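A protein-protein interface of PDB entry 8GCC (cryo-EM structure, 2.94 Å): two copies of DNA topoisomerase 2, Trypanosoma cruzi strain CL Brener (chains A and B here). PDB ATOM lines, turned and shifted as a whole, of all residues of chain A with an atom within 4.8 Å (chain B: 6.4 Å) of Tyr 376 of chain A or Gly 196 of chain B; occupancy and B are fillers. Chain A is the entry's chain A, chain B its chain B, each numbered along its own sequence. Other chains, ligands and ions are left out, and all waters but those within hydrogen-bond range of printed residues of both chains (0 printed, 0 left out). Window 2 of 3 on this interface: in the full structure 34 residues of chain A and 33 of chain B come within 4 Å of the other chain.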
ATOM      1  N   ASP A 358     -21.624   6.680  -9.390  1.00  0.00           N
ATOM      2  CA  ASP A 358     -21.137   7.721  -8.483  1.00  0.00           C
ATOM      3  C   ASP A 358     -21.985   8.964  -8.748  1.00  0.00           C
ATOM      4  O   ASP A 358     -21.676   9.763  -9.637  1.00  0.00           O
ATOM      5  CB  ASP A 358     -19.654   7.990  -8.695  1.00  0.00           C
ATOM      6  N   GLN A 360     -26.354  10.482  -8.406  1.00  0.00           N
ATOM      7  CA  GLN A 360     -27.773  10.164  -8.254  1.00  0.00           C
ATOM      8  C   GLN A 360     -28.217   9.396  -9.494  1.00  0.00           C
ATOM      9  O   GLN A 360     -28.603   9.980 -10.505  1.00  0.00           O
ATOM     10  CB  GLN A 360     -28.599  11.430  -8.063  1.00  0.00           C
ATOM     11  CG  GLN A 360     -28.077  12.366  -6.992  1.00  0.00           C
ATOM     12  CD  GLN A 360     -28.922  13.616  -6.855  1.00  0.00           C
ATOM     13  N   ALA A 372     -29.896  12.211 -11.607  1.00  0.00           N
ATOM     14  CA  ALA A 372     -29.372  13.477 -12.088  1.00  0.00           C
ATOM     15  C   ALA A 372     -29.025  13.379 -13.572  1.00  0.00           C
ATOM     16  O   ALA A 372     -28.931  12.295 -14.151  1.00  0.00           O
ATOM     17  CB  ALA A 372     -28.143  13.888 -11.278  1.00  0.00           C
ATOM     18  N   ALA A 373     -28.838  14.542 -14.188  1.00  0.00           N
ATOM     19  CA  ALA A 373     -28.485  14.592 -15.597  1.00  0.00           C
ATOM     20  C   ALA A 373     -27.120  13.952 -15.823  1.00  0.00           C
ATOM     21  O   ALA A 373     -26.287  13.862 -14.919  1.00  0.00           O
ATOM     22  CB  ALA A 373     -28.478  16.036 -16.092  1.00  0.00           C
ATOM     23  N   GLY A 374     -26.893  13.505 -17.059  1.00  0.00           N
ATOM     24  CA  GLY A 374     -25.657  12.808 -17.368  1.00  0.00           C
ATOM     25  C   GLY A 374     -24.419  13.625 -17.060  1.00  0.00           C
ATOM     26  O   GLY A 374     -23.344  13.066 -16.826  1.00  0.00           O
ATOM     27  N   ARG A 375     -24.546  14.951 -17.058  1.00  0.00           N
ATOM     28  CA  ARG A 375     -23.426  15.824 -16.736  1.00  0.00           C
ATOM     29  C   ARG A 375     -23.063  15.803 -15.258  1.00  0.00           C
ATOM     30  O   ARG A 375     -22.021  16.351 -14.890  1.00  0.00           O
ATOM     31  CB  ARG A 375     -23.747  17.258 -17.159  1.00  0.00           C
ATOM     32  CG  ARG A 375     -24.924  17.871 -16.412  1.00  0.00           C
ATOM     33  CD  ARG A 375     -25.394  19.163 -17.056  1.00  0.00           C
ATOM     34  NE  ARG A 375     -24.839  20.337 -16.388  1.00  0.00           N
ATOM     35  CZ  ARG A 375     -23.896  21.123 -16.889  1.00  0.00           C
ATOM     36  NH1 ARG A 375     -23.345  20.887 -18.069  1.00  0.00           N
ATOM     37  NH2 ARG A 375     -23.488  22.176 -16.186  1.00  0.00           N
ATOM     38  N   TYR A 376     -23.893  15.199 -14.406  1.00  0.00           N
ATOM     39  CA  TYR A 376     -23.653  15.187 -12.971  1.00  0.00           C
ATOM     40  C   TYR A 376     -23.339  13.812 -12.405  1.00  0.00           C
ATOM     41  O   TYR A 376     -22.846  13.732 -11.276  1.00  0.00           O
ATOM     42  CB  TYR A 376     -24.874  15.746 -12.225  1.00  0.00           C
ATOM     43  CG  TYR A 376     -25.149  17.213 -12.464  1.00  0.00           C
ATOM     44  CD1 TYR A 376     -26.425  17.728 -12.307  1.00  0.00           C
ATOM     45  CD2 TYR A 376     -24.133  18.088 -12.826  1.00  0.00           C
ATOM     46  CE1 TYR A 376     -26.686  19.065 -12.515  1.00  0.00           C
ATOM     47  CE2 TYR A 376     -24.384  19.427 -13.036  1.00  0.00           C
ATOM     48  CZ  TYR A 376     -25.663  19.910 -12.877  1.00  0.00           C
ATOM     49  OH  TYR A 376     -25.921  21.246 -13.084  1.00  0.00           O
ATOM     50  N   ILE A 377     -23.600  12.742 -13.147  1.00  0.00           N
ATOM     51  CA  ILE A 377     -23.410  11.380 -12.656  1.00  0.00           C
ATOM     52  C   ILE A 377     -22.175  10.789 -13.314  1.00  0.00           C
ATOM     53  O   ILE A 377     -21.960  10.947 -14.521  1.00  0.00           O
ATOM     54  CB  ILE A 377     -24.649  10.500 -12.917  1.00  0.00           C
ATOM     55  CG1 ILE A 377     -25.232  10.760 -14.306  1.00  0.00           C
ATOM     56  CG2 ILE A 377     -25.704  10.750 -11.865  1.00  0.00           C
ATOM     57  CD1 ILE A 377     -26.382   9.845 -14.661  1.00  0.00           C
ATOM     58  N   PHE A 378     -21.356  10.117 -12.514  1.00  0.00           N
ATOM     59  CA  PHE A 378     -20.159   9.440 -12.985  1.00  0.00           C
ATOM     60  C   PHE A 378     -20.377   7.934 -12.925  1.00  0.00           C
ATOM     61  O   PHE A 378     -21.189   7.442 -12.141  1.00  0.00           O
ATOM     62  CB  PHE A 378     -18.941   9.819 -12.138  1.00  0.00           C
ATOM     63  CG  PHE A 378     -18.499  11.243 -12.310  1.00  0.00           C
ATOM     64  CD1 PHE A 378     -19.340  12.290 -11.980  1.00  0.00           C
ATOM     65  CD2 PHE A 378     -17.241  11.534 -12.796  1.00  0.00           C
ATOM     66  CE1 PHE A 378     -18.936  13.595 -12.137  1.00  0.00           C
ATOM     67  CE2 PHE A 378     -16.833  12.837 -12.954  1.00  0.00           C
ATOM     68  CZ  PHE A 378     -17.683  13.869 -12.625  1.00  0.00           C
ATOM     69  N   SER B  38     -31.808  20.318  -9.150  1.00  0.00           N
ATOM     70  CA  SER B  38     -30.801  19.621  -8.357  1.00  0.00           C
ATOM     71  C   SER B  38     -30.875  20.034  -6.892  1.00  0.00           C
ATOM     72  O   SER B  38     -30.864  19.185  -5.988  1.00  0.00           O
ATOM     73  CB  SER B  38     -29.413  19.901  -8.928  1.00  0.00           C
ATOM     74  N   ALA B  39     -30.955  21.340  -6.635  1.00  0.00           N
ATOM     75  CA  ALA B  39     -31.090  21.806  -5.262  1.00  0.00           C
ATOM     76  C   ALA B  39     -32.408  21.355  -4.653  1.00  0.00           C
ATOM     77  O   ALA B  39     -32.474  21.100  -3.449  1.00  0.00           O
ATOM     78  CB  ALA B  39     -30.968  23.327  -5.202  1.00  0.00           C
ATOM     79  N   LYS B 193     -18.822  19.112  -7.980  1.00  0.00           N
ATOM     80  CA  LYS B 193     -18.784  20.360  -8.735  1.00  0.00           C
ATOM     81  C   LYS B 193     -20.176  20.966  -8.862  1.00  0.00           C
ATOM     82  O   LYS B 193     -20.447  22.051  -8.334  1.00  0.00           O
ATOM     83  CB  LYS B 193     -18.176  20.112 -10.116  1.00  0.00           C
ATOM     84  N   GLY B 194     -21.075  20.278  -9.557  1.00  0.00           N
ATOM     85  CA  GLY B 194     -22.439  20.744  -9.648  1.00  0.00           C
ATOM     86  C   GLY B 194     -23.209  20.500  -8.367  1.00  0.00           C
ATOM     87  O   GLY B 194     -22.873  19.636  -7.560  1.00  0.00           O
ATOM     88  N   LEU B 195     -24.268  21.283  -8.176  1.00  0.00           N
ATOM     89  CA  LEU B 195     -25.085  21.129  -6.983  1.00  0.00           C
ATOM     90  C   LEU B 195     -26.010  19.923  -7.054  1.00  0.00           C
ATOM     91  O   LEU B 195     -26.575  19.535  -6.027  1.00  0.00           O
ATOM     92  CB  LEU B 195     -25.908  22.393  -6.737  1.00  0.00           C
ATOM     93  CG  LEU B 195     -26.435  22.519  -5.308  1.00  0.00           C
ATOM     94  CD1 LEU B 195     -26.151  23.897  -4.745  1.00  0.00           C
ATOM     95  CD2 LEU B 195     -27.910  22.227  -5.271  1.00  0.00           C
ATOM     96  N   GLY B 196     -26.182  19.329  -8.231  1.00  0.00           N
ATOM     97  CA  GLY B 196     -26.927  18.100  -8.384  1.00  0.00           C
ATOM     98  C   GLY B 196     -26.116  16.845  -8.184  1.00  0.00           C
ATOM     99  O   GLY B 196     -26.662  15.743  -8.288  1.00  0.00           O
ATOM    100  N   THR B 197     -24.822  16.976  -7.900  1.00  0.00           N
ATOM    101  CA  THR B 197     -23.958  15.824  -7.689  1.00  0.00           C
ATOM    102  C   THR B 197     -24.112  15.215  -6.302  1.00  0.00           C
ATOM    103  O   THR B 197     -23.524  14.161  -6.039  1.00  0.00           O
ATOM    104  CB  THR B 197     -22.497  16.224  -7.909  1.00  0.00           C
ATOM    105  OG1 THR B 197     -22.408  17.123  -9.021  1.00  0.00           O
ATOM    106  CG2 THR B 197     -21.638  15.000  -8.183  1.00  0.00           C
ATOM    107  N   SER B 198     -24.882  15.844  -5.420  1.00  0.00           N
ATOM    108  CA  SER B 198     -25.084  15.368  -4.060  1.00  0.00           C
ATOM    109  C   SER B 198     -26.468  14.750  -3.939  1.00  0.00           C
ATOM    110  O   SER B 198     -27.459  15.346  -4.374  1.00  0.00           O
ATOM    111  CB  SER B 198     -24.924  16.511  -3.058  1.00  0.00           C
ATOM    112  OG  SER B 198     -25.478  17.709  -3.571  1.00  0.00           O
ATOM    113  N   GLY B 199     -26.531  13.560  -3.345  1.00  0.00           N
ATOM    114  CA  GLY B 199     -27.782  12.843  -3.196  1.00  0.00           C
ATOM    115  C   GLY B 199     -28.491  13.128  -1.888  1.00  0.00           C
ATOM    116  O   GLY B 199     -28.597  14.285  -1.471  1.00  0.00           O
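The backbone NH (N) of Ala 372 of chain A sits at hydrogen-bond distance from the backbone carbonyl oxygen (O) of Gln 360 of chain A (2.8 Å).
O of Gly 194 of chain B is in hydrogen-bond range of OG1 of Thr 197 of chain B, 2.9 Å away.
O of Leu 195 of chain B is in hydrogen-bond range of OG of Ser 198 of chain B (3.3 Å).
Printed residues of chain B within 4 Å of Gln 360 of chain A: Gly 196, Ser 198 and Gly 199.
Of the printed residues of chain B, Ala 372 of chain A touches Gly 196 (3.8 Å).
Of chain B, only Gly 196 and Thr 197 come within 4 Å of Tyr 376 of chain A.
Of the printed residues of chain A, Thr 197 of chain B touches Tyr 376 (3.6 Å).
Printed residues of chain A within 4 Å of Gly 199 of chain B: Gln 360.
The nearest printed residue of chain A that does not touch Gly 196 of chain B is Ile 377 of chain A (6.2 Å).
The nearest printed residue of chain B that does not touch Ala 372 of chain A is Thr 197 of chain B (5.7 Å).
No position is printed for both chains.
O of Gly 196 of chain B touches CD of Gln 360 of chain A, 3.4 Å away.
Ser 198 of chain B touches Gln 360 of chain A (O to CD, 3.4 Å).
Gln 360 of chain A touches Gly 199 of chain B.
CB of Ala 372 of chain A touches O of Gly 196 of chain B, 3.8 Å away.
CD1 of Tyr 376 of chain A touches CA of Gly 196 of chain B (3.97 Å).
Tyr 376 of chain A touches Thr 197 of chain B (O to CG2, 3.6 Å).
Of the 9 printed residues of chain A, 3 touch a printed residue of chain B.
Printed residues of chain A that touch a printed residue of chain B: Gln 360, Ala 372 and Tyr 376.
Hydrophobic or aromatic side chains of chain A within 4 Å of the printed part of chain B: Ala 372 and Tyr 376.
Along chain B the printed residues that touch a printed residue of chain A span positions 196 to 199.
Among the printed residues, 6 pairs touch across the chains.
Among the printed residues, no Asp or Glu carboxylate lies within 4 Å of a Lys or Arg side-chain nitrogen of the other chain.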
